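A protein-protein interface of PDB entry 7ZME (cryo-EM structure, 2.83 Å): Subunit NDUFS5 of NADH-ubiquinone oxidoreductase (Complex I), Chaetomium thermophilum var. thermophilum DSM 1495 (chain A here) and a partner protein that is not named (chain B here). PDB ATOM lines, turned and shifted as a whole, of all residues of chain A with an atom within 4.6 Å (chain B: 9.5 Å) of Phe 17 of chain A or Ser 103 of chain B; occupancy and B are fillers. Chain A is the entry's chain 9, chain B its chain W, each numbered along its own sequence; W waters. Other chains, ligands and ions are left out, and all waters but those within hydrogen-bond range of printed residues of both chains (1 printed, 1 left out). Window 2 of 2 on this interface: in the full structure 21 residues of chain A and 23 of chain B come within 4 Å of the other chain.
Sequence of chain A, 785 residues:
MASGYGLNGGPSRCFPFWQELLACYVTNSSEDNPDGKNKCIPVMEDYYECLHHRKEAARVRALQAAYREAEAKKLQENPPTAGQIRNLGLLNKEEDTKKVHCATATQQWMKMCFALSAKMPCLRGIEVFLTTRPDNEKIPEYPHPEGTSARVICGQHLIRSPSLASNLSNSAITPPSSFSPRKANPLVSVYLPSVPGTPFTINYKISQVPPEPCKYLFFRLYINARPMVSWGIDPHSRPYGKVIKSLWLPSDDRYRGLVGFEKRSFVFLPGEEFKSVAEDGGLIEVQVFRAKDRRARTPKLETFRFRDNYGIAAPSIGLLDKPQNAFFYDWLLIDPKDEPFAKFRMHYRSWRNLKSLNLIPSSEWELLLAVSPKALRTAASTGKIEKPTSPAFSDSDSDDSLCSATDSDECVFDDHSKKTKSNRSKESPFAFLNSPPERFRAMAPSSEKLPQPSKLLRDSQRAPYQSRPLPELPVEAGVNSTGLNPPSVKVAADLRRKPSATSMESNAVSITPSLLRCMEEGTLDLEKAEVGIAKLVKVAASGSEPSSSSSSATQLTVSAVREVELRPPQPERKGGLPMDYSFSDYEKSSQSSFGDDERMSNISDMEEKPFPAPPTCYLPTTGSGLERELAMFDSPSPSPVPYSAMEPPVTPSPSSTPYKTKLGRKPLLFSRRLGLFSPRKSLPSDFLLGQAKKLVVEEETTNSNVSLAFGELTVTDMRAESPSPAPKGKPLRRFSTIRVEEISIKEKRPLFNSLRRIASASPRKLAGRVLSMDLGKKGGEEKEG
Printed residues of chain B that touch a printed residue of chain A: Tyr 101, Asn 102, Ser 103, Arg 105 and Val 107. Along chain B the printed residues that touch a printed residue of chain A span positions 101 to 107.
Of the printed residues of chain B, Phe 17 of chain A touches Tyr 101 (3.7 Å), Ser 103 (3.7 Å), Arg 105 (3.5 Å) and Val 107 (3.7 Å). Printed residues of chain A within 4 Å of Ser 103 of chain B: Phe 17 and Asp 46. Of the printed residues of chain B, Pro 16 of chain A touches Arg 105 (3.3 Å). Glu 20 of chain A touches none of the printed residues of chain B. Printed residues of chain A within 4 Å of Val 107 of chain B: Phe 17 (3.7 Å). Of the printed residues of chain A, Tyr 101 of chain B touches Phe 17 (3.7 Å), Asp 46 (3.6 Å) and Cys 50 (3.2 Å). Of the printed residues of chain A, Asn 102 of chain B touches Asp 46 (2.8 Å). Of the printed residues of chain A, Arg 105 of chain B touches Pro 16 (3.3 Å) and Phe 17 (3.5 Å). Trp 18 of chain A touches none of the printed residues of chain B. The nearest residue of chain B that does not touch Phe 17 of chain A is Tyr 106 of chain B (6.1 Å). The nearest printed residue of chain A that does not touch Ser 103 of chain B is Glu 20 of chain A (4.8 Å).
Water W1 lies within hydrogen-bond range of the side-chain hydroxyl of Tyr 101 of chain B (2.6 Å) and the backbone carbonyl oxygen of Cys 50 of chain A (3.4 Å).
CB of Pro 16 of chain A touches NH2 of Arg 105 of chain B, 3.3 Å away. Tyr 101 of chain B touches Phe 17 of chain A (CE1 to CZ, 3.7 Å). Ser 103 of chain B touches Phe 17 of chain A. Phe 17 of chain A touches Arg 105 of chain B. Phe 17 of chain A touches Val 107 of chain B. Asp 46 of chain A touches Tyr 101 of chain B (O to CE1, 3.6 Å).
The backbone NH (N) of Cys 50 of chain A lies close to the side-chain hydroxyl (OH) of Tyr 101 of chain B (3.3 Å). N of Ser 103 of chain B lies within hydrogen-bond range of OD2 of Asp 46 of chain A, at 3.3 Å. The backbone NH (N) of Asn 102 of chain B sits at hydrogen-bond distance from the side-chain carboxylate (OD1) of Asp 46 of chain A (2.8 Å).
The side-chain sulfur (SG) of Cys 50 of chain A is disulfide-bonded to the side-chain sulfur (SG) of Cys 14 of chain A, at 2.0 Å.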
ATOM      1  N   CYS A  14      -2.377  19.387  -9.675  1.00  0.00           N
ATOM      2  CA  CYS A  14      -2.952  19.622 -11.024  1.00  0.00           C
ATOM      3  C   CYS A  14      -3.681  20.962 -11.063  1.00  0.00           C
ATOM      4  O   CYS A  14      -4.534  21.116 -11.926  1.00  0.00           O
ATOM      5  CB  CYS A  14      -3.879  18.474 -11.412  1.00  0.00           C
ATOM      6  SG  CYS A  14      -2.988  16.921 -11.635  1.00  0.00           S
ATOM      7  N   PHE A  15      -3.353  21.876 -10.158  1.00  0.00           N
ATOM      8  CA  PHE A  15      -3.991  23.182 -10.212  1.00  0.00           C
ATOM      9  C   PHE A  15      -3.422  24.082 -11.307  1.00  0.00           C
ATOM     10  O   PHE A  15      -4.197  24.785 -11.965  1.00  0.00           O
ATOM     11  CB  PHE A  15      -3.895  23.880  -8.858  1.00  0.00           C
ATOM     12  CG  PHE A  15      -4.801  25.062  -8.735  1.00  0.00           C
ATOM     13  CD1 PHE A  15      -6.154  24.937  -8.991  1.00  0.00           C
ATOM     14  CD2 PHE A  15      -4.302  26.300  -8.383  1.00  0.00           C
ATOM     15  CE1 PHE A  15      -6.987  26.022  -8.890  1.00  0.00           C
ATOM     16  CE2 PHE A  15      -5.135  27.385  -8.279  1.00  0.00           C
ATOM     17  CZ  PHE A  15      -6.478  27.246  -8.529  1.00  0.00           C
ATOM     18  N   PRO A  16      -2.086  24.125 -11.567  1.00  0.00           N
ATOM     19  CA  PRO A  16      -1.564  24.898 -12.694  1.00  0.00           C
ATOM     20  C   PRO A  16      -2.159  24.426 -14.027  1.00  0.00           C
ATOM     21  O   PRO A  16      -2.467  25.251 -14.832  1.00  0.00           O
ATOM     22  CB  PRO A  16      -0.074  24.563 -12.676  1.00  0.00           C
ATOM     23  CG  PRO A  16       0.235  24.302 -11.247  1.00  0.00           C
ATOM     24  CD  PRO A  16      -0.969  23.517 -10.805  1.00  0.00           C
ATOM     25  N   PHE A  17      -2.309  23.118 -14.210  1.00  0.00           N
ATOM     26  CA  PHE A  17      -2.879  22.527 -15.441  1.00  0.00           C
ATOM     27  C   PHE A  17      -4.337  22.952 -15.604  1.00  0.00           C
ATOM     28  O   PHE A  17      -4.784  23.117 -16.743  1.00  0.00           O
ATOM     29  CB  PHE A  17      -2.655  21.016 -15.420  1.00  0.00           C
ATOM     30  CG  PHE A  17      -1.287  20.587 -15.882  1.00  0.00           C
ATOM     31  CD1 PHE A  17      -0.936  20.667 -17.218  1.00  0.00           C
ATOM     32  CD2 PHE A  17      -0.350  20.104 -14.985  1.00  0.00           C
ATOM     33  CE1 PHE A  17       0.320  20.269 -17.646  1.00  0.00           C
ATOM     34  CE2 PHE A  17       0.903  19.703 -15.414  1.00  0.00           C
ATOM     35  CZ  PHE A  17       1.235  19.786 -16.743  1.00  0.00           C
ATOM     36  N   TRP A  18      -5.063  23.122 -14.502  1.00  0.00           N
ATOM     37  CA  TRP A  18      -6.498  23.503 -14.542  1.00  0.00           C
ATOM     38  C   TRP A  18      -6.630  25.003 -14.805  1.00  0.00           C
ATOM     39  O   TRP A  18      -7.498  25.390 -15.590  1.00  0.00           O
ATOM     40  CB  TRP A  18      -7.140  23.114 -13.210  1.00  0.00           C
ATOM     41  CG  TRP A  18      -8.562  23.548 -13.046  1.00  0.00           C
ATOM     42  CD1 TRP A  18      -9.032  24.530 -12.225  1.00  0.00           C
ATOM     43  CD2 TRP A  18      -9.710  23.002 -13.718  1.00  0.00           C
ATOM     44  NE1 TRP A  18     -10.391  24.631 -12.338  1.00  0.00           N
ATOM     45  CE2 TRP A  18     -10.835  23.710 -13.249  1.00  0.00           C
ATOM     46  CE3 TRP A  18      -9.896  21.992 -14.667  1.00  0.00           C
ATOM     47  CZ2 TRP A  18     -12.125  23.435 -13.694  1.00  0.00           C
ATOM     48  CZ3 TRP A  18     -11.171  21.718 -15.104  1.00  0.00           C
ATOM     49  CH2 TRP A  18     -12.268  22.431 -14.626  1.00  0.00           C
ATOM     50  N   GLN A  19      -5.791  25.813 -14.171  1.00  0.00           N
ATOM     51  CA  GLN A  19      -5.851  27.287 -14.318  1.00  0.00           C
ATOM     52  C   GLN A  19      -5.478  27.642 -15.752  1.00  0.00           C
ATOM     53  O   GLN A  19      -6.079  28.571 -16.290  1.00  0.00           O
ATOM     54  CB  GLN A  19      -5.002  27.974 -13.247  1.00  0.00           C
ATOM     55  CG  GLN A  19      -5.590  27.872 -11.855  1.00  0.00           C
ATOM     56  CD  GLN A  19      -6.399  29.085 -11.472  1.00  0.00           C
ATOM     57  OE1 GLN A  19      -5.856  30.149 -11.196  1.00  0.00           O
ATOM     58  NE2 GLN A  19      -7.712  28.925 -11.422  1.00  0.00           N
ATOM     59  N   GLU A  20      -4.539  26.914 -16.340  1.00  0.00           N
ATOM     60  CA  GLU A  20      -4.174  27.160 -17.754  1.00  0.00           C
ATOM     61  C   GLU A  20      -5.344  26.831 -18.690  1.00  0.00           C
ATOM     62  O   GLU A  20      -5.567  27.588 -19.630  1.00  0.00           O
ATOM     63  CB  GLU A  20      -2.868  26.444 -18.104  1.00  0.00           C
ATOM     64  CG  GLU A  20      -2.376  26.754 -19.504  1.00  0.00           C
ATOM     65  CD  GLU A  20      -1.239  25.873 -19.981  1.00  0.00           C
ATOM     66  OE1 GLU A  20      -0.780  26.067 -21.122  1.00  0.00           O
ATOM     67  OE2 GLU A  20      -0.815  24.995 -19.207  1.00  0.00           O
ATOM     68  N   LEU A  21      -6.046  25.736 -18.452  1.00  0.00           N
ATOM     69  CA  LEU A  21      -7.193  25.346 -19.299  1.00  0.00           C
ATOM     70  C   LEU A  21      -8.330  26.368 -19.216  1.00  0.00           C
ATOM     71  O   LEU A  21      -8.879  26.719 -20.274  1.00  0.00           O
ATOM     72  CB  LEU A  21      -7.649  23.963 -18.839  1.00  0.00           C
ATOM     73  CG  LEU A  21      -8.826  23.354 -19.586  1.00  0.00           C
ATOM     74  CD1 LEU A  21      -8.526  23.272 -21.072  1.00  0.00           C
ATOM     75  CD2 LEU A  21      -9.154  21.984 -19.020  1.00  0.00           C
ATOM     76  N   VAL A  43      -4.567  21.631 -24.151  1.00  0.00           N
ATOM     77  CA  VAL A  43      -4.554  22.099 -22.772  1.00  0.00           C
ATOM     78  C   VAL A  43      -5.437  21.218 -21.899  1.00  0.00           C
ATOM     79  O   VAL A  43      -5.122  20.967 -20.730  1.00  0.00           O
ATOM     80  CB  VAL A  43      -4.990  23.574 -22.728  1.00  0.00           C
ATOM     81  CG1 VAL A  43      -4.693  24.172 -21.391  1.00  0.00           C
ATOM     82  CG2 VAL A  43      -4.288  24.354 -23.815  1.00  0.00           C
ATOM     83  N   ASP A  46      -3.668  17.848 -21.232  1.00  0.00           N
ATOM     84  CA  ASP A  46      -2.621  17.937 -20.221  1.00  0.00           C
ATOM     85  C   ASP A  46      -3.202  17.879 -18.818  1.00  0.00           C
ATOM     86  O   ASP A  46      -2.578  17.330 -17.904  1.00  0.00           O
ATOM     87  CB  ASP A  46      -1.820  19.223 -20.405  1.00  0.00           C
ATOM     88  CG  ASP A  46      -1.037  19.240 -21.687  1.00  0.00           C
ATOM     89  OD1 ASP A  46      -0.768  18.153 -22.229  1.00  0.00           O
ATOM     90  OD2 ASP A  46      -0.689  20.339 -22.155  1.00  0.00           O
ATOM     91  N   TYR A  47      -4.382  18.469 -18.622  1.00  0.00           N
ATOM     92  CA  TYR A  47      -5.022  18.424 -17.314  1.00  0.00           C
ATOM     93  C   TYR A  47      -5.417  17.001 -16.947  1.00  0.00           C
ATOM     94  O   TYR A  47      -5.234  16.575 -15.802  1.00  0.00           O
ATOM     95  CB  TYR A  47      -6.238  19.350 -17.292  1.00  0.00           C
ATOM     96  CG  TYR A  47      -7.116  19.158 -16.080  1.00  0.00           C
ATOM     97  CD1 TYR A  47      -6.695  19.564 -14.824  1.00  0.00           C
ATOM     98  CD2 TYR A  47      -8.355  18.550 -16.189  1.00  0.00           C
ATOM     99  CE1 TYR A  47      -7.487  19.381 -13.717  1.00  0.00           C
ATOM    100  CE2 TYR A  47      -9.150  18.362 -15.089  1.00  0.00           C
ATOM    101  CZ  TYR A  47      -8.714  18.780 -13.854  1.00  0.00           C
ATOM    102  OH  TYR A  47      -9.515  18.594 -12.754  1.00  0.00           O
ATOM    103  N   CYS A  50      -2.072  15.109 -16.193  1.00  0.00           N
ATOM    104  CA  CYS A  50      -1.657  15.398 -14.824  1.00  0.00           C
ATOM    105  C   CYS A  50      -2.478  14.605 -13.825  1.00  0.00           C
ATOM    106  O   CYS A  50      -1.976  14.211 -12.770  1.00  0.00           O
ATOM    107  CB  CYS A  50      -1.797  16.895 -14.539  1.00  0.00           C
ATOM    108  SG  CYS A  50      -1.428  17.454 -12.840  1.00  0.00           S
ATOM    109  N   TYR B  83      16.169  14.250 -15.393  1.00  0.00           N
ATOM    110  CA  TYR B  83      15.293  14.439 -16.572  1.00  0.00           C
ATOM    111  C   TYR B  83      16.157  14.297 -17.817  1.00  0.00           C
ATOM    112  O   TYR B  83      15.776  13.536 -18.713  1.00  0.00           O
ATOM    113  CB  TYR B  83      14.568  15.785 -16.533  1.00  0.00           C
ATOM    114  CG  TYR B  83      13.740  16.090 -17.756  1.00  0.00           C
ATOM    115  CD1 TYR B  83      14.286  16.738 -18.851  1.00  0.00           C
ATOM    116  CD2 TYR B  83      12.408  15.726 -17.821  1.00  0.00           C
ATOM    117  CE1 TYR B  83      13.532  17.020 -19.976  1.00  0.00           C
ATOM    118  CE2 TYR B  83      11.639  15.997 -18.939  1.00  0.00           C
ATOM    119  CZ  TYR B  83      12.203  16.646 -20.021  1.00  0.00           C
ATOM    120  OH  TYR B  83      11.451  16.917 -21.126  1.00  0.00           O
ATOM    121  N   ILE B  98       9.097  10.226 -26.468  1.00  0.00           N
ATOM    122  CA  ILE B  98       7.603  10.250 -26.501  1.00  0.00           C
ATOM    123  C   ILE B  98       7.129  11.456 -25.691  1.00  0.00           C
ATOM    124  O   ILE B  98       7.687  11.683 -24.602  1.00  0.00           O
ATOM    125  CB  ILE B  98       7.015   8.938 -25.946  1.00  0.00           C
ATOM    126  CG1 ILE B  98       7.540   7.714 -26.698  1.00  0.00           C
ATOM    127  CG2 ILE B  98       5.494   8.980 -25.944  1.00  0.00           C
ATOM    128  CD1 ILE B  98       6.956   7.555 -28.079  1.00  0.00           C
ATOM    129  N   LYS B  99       6.153  12.202 -26.208  1.00  0.00           N
ATOM    130  CA  LYS B  99       5.692  13.433 -25.514  1.00  0.00           C
ATOM    131  C   LYS B  99       4.483  13.105 -24.637  1.00  0.00           C
ATOM    132  O   LYS B  99       3.384  12.950 -25.191  1.00  0.00           O
ATOM    133  CB  LYS B  99       5.314  14.489 -26.556  1.00  0.00           C
ATOM    134  CG  LYS B  99       5.348  15.930 -26.072  1.00  0.00           C
ATOM    135  CD  LYS B  99       6.706  16.365 -25.563  1.00  0.00           C
ATOM    136  CE  LYS B  99       7.747  16.471 -26.657  1.00  0.00           C
ATOM    137  NZ  LYS B  99       9.034  16.990 -26.138  1.00  0.00           N
ATOM    138  N   VAL B 100       4.688  12.986 -23.329  1.00  0.00           N
ATOM    139  CA  VAL B 100       3.553  12.756 -22.392  1.00  0.00           C
ATOM    140  C   VAL B 100       2.688  14.013 -22.312  1.00  0.00           C
ATOM    141  O   VAL B 100       1.460  13.875 -22.276  1.00  0.00           O
ATOM    142  CB  VAL B 100       4.045  12.308 -21.005  1.00  0.00           C
ATOM    143  CG1 VAL B 100       2.903  12.131 -20.022  1.00  0.00           C
ATOM    144  CG2 VAL B 100       4.884  11.044 -21.092  1.00  0.00           C
ATOM    145  N   TYR B 101       3.303  15.194 -22.271  1.00  0.00           N
ATOM    146  CA  TYR B 101       2.502  16.429 -22.090  1.00  0.00           C
ATOM    147  C   TYR B 101       2.679  17.329 -23.298  1.00  0.00           C
ATOM    148  O   TYR B 101       3.789  17.410 -23.817  1.00  0.00           O
ATOM    149  CB  TYR B 101       2.891  17.198 -20.828  1.00  0.00           C
ATOM    150  CG  TYR B 101       2.453  16.560 -19.537  1.00  0.00           C
ATOM    151  CD1 TYR B 101       1.225  16.863 -18.976  1.00  0.00           C
ATOM    152  CD2 TYR B 101       3.268  15.661 -18.876  1.00  0.00           C
ATOM    153  CE1 TYR B 101       0.815  16.286 -17.788  1.00  0.00           C
ATOM    154  CE2 TYR B 101       2.870  15.067 -17.693  1.00  0.00           C
ATOM    155  CZ  TYR B 101       1.641  15.383 -17.147  1.00  0.00           C
ATOM    156  OH  TYR B 101       1.252  14.801 -15.980  1.00  0.00           O
ATOM    157  N   ASN B 102       1.607  18.001 -23.699  1.00  0.00           N
ATOM    158  CA  ASN B 102       1.684  18.925 -24.822  1.00  0.00           C
ATOM    159  C   ASN B 102       2.461  20.180 -24.457  1.00  0.00           C
ATOM    160  O   ASN B 102       3.120  20.773 -25.317  1.00  0.00           O
ATOM    161  CB  ASN B 102       0.278  19.284 -25.293  1.00  0.00           C
ATOM    162  CG  ASN B 102      -0.493  18.081 -25.777  1.00  0.00           C
ATOM    163  OD1 ASN B 102      -0.058  17.380 -26.686  1.00  0.00           O
ATOM    164  ND2 ASN B 102      -1.643  17.832 -25.171  1.00  0.00           N
ATOM    165  N   SER B 103       2.403  20.591 -23.197  1.00  0.00           N
ATOM    166  CA  SER B 103       3.084  21.792 -22.752  1.00  0.00           C
ATOM    167  C   SER B 103       4.581  21.540 -22.586  1.00  0.00           C
ATOM    168  O   SER B 103       5.047  20.401 -22.504  1.00  0.00           O
ATOM    169  CB  SER B 103       2.483  22.286 -21.440  1.00  0.00           C
ATOM    170  OG  SER B 103       2.558  21.286 -20.445  1.00  0.00           O
ATOM    171  N   ASP B 104       5.336  22.633 -22.543  1.00  0.00           N
ATOM    172  CA  ASP B 104       6.782  22.587 -22.391  1.00  0.00           C
ATOM    173  C   ASP B 104       7.214  22.540 -20.933  1.00  0.00           C
ATOM    174  O   ASP B 104       8.410  22.412 -20.655  1.00  0.00           O
ATOM    175  CB  ASP B 104       7.410  23.800 -23.090  1.00  0.00           C
ATOM    176  CG  ASP B 104       8.919  23.701 -23.203  1.00  0.00           C
ATOM    177  OD1 ASP B 104       9.402  22.919 -24.049  1.00  0.00           O
ATOM    178  OD2 ASP B 104       9.620  24.406 -22.449  1.00  0.00           O
ATOM    179  N   ARG B 105       6.254  22.545 -19.999  1.00  0.00           N
ATOM    180  CA  ARG B 105       6.585  22.647 -18.552  1.00  0.00           C
ATOM    181  C   ARG B 105       7.170  21.363 -17.969  1.00  0.00           C
ATOM    182  O   ARG B 105       6.692  20.292 -18.314  1.00  0.00           O
ATOM    183  CB  ARG B 105       5.341  23.038 -17.759  1.00  0.00           C
ATOM    184  CG  ARG B 105       4.150  22.107 -17.910  1.00  0.00           C
ATOM    185  CD  ARG B 105       2.981  22.805 -17.257  1.00  0.00           C
ATOM    186  NE  ARG B 105       3.388  23.249 -15.935  1.00  0.00           N
ATOM    187  CZ  ARG B 105       2.668  24.033 -15.151  1.00  0.00           C
ATOM    188  NH1 ARG B 105       3.127  24.379 -13.963  1.00  0.00           N
ATOM    189  NH2 ARG B 105       1.496  24.477 -15.565  1.00  0.00           N
ATOM    190  N   TYR B 106       8.140  21.489 -17.058  1.00  0.00           N
ATOM    191  CA  TYR B 106       8.677  20.280 -16.397  1.00  0.00           C
ATOM    192  C   TYR B 106       7.603  19.685 -15.495  1.00  0.00           C
ATOM    193  O   TYR B 106       6.985  20.441 -14.733  1.00  0.00           O
ATOM    194  CB  TYR B 106       9.887  20.600 -15.519  1.00  0.00           C
ATOM    195  CG  TYR B 106      10.396  19.412 -14.746  1.00  0.00           C
ATOM    196  CD1 TYR B 106      10.790  18.261 -15.405  1.00  0.00           C
ATOM    197  CD2 TYR B 106      10.461  19.426 -13.363  1.00  0.00           C
ATOM    198  CE1 TYR B 106      11.246  17.154 -14.713  1.00  0.00           C
ATOM    199  CE2 TYR B 106      10.916  18.325 -12.656  1.00  0.00           C
ATOM    200  CZ  TYR B 106      11.311  17.187 -13.334  1.00  0.00           C
ATOM    201  OH  TYR B 106      11.766  16.091 -12.666  1.00  0.00           O
ATOM    202  N   VAL B 107       7.402  18.371 -15.578  1.00  0.00           N
ATOM    203  CA  VAL B 107       6.457  17.722 -14.638  1.00  0.00           C
ATOM    204  C   VAL B 107       7.241  16.682 -13.831  1.00  0.00           C
ATOM    205  O   VAL B 107       7.905  15.833 -14.446  1.00  0.00           O
ATOM    206  CB  VAL B 107       5.216  17.148 -15.351  1.00  0.00           C
ATOM    207  CG1 VAL B 107       4.183  16.635 -14.362  1.00  0.00           C
ATOM    208  CG2 VAL B 107       4.581  18.158 -16.294  1.00  0.00           C
ATOM    209  N   ARG B 108       7.252  16.781 -12.502  1.00  0.00           N
ATOM    210  CA  ARG B 108       7.956  15.756 -11.693  1.00  0.00           C
ATOM    211  C   ARG B 108       7.392  14.368 -12.009  1.00  0.00           C
ATOM    212  O   ARG B 108       6.168  14.187 -11.915  1.00  0.00           O
ATOM    213  CB  ARG B 108       7.842  16.106 -10.207  1.00  0.00           C
ATOM    214  CG  ARG B 108       8.814  17.187  -9.765  1.00  0.00           C
ATOM    215  CD  ARG B 108       8.277  18.026  -8.627  1.00  0.00           C
ATOM    216  NE  ARG B 108       9.175  19.115  -8.271  1.00  0.00           N
ATOM    217  CZ  ARG B 108       9.097  20.349  -8.754  1.00  0.00           C
ATOM    218  NH1 ARG B 108       9.958  21.270  -8.359  1.00  0.00           N
ATOM    219  NH2 ARG B 108       8.157  20.662  -9.625  1.00  0.00           N
HETATM  220  O   HOH W   1       1.333  14.626 -13.401  1.00  0.00           O
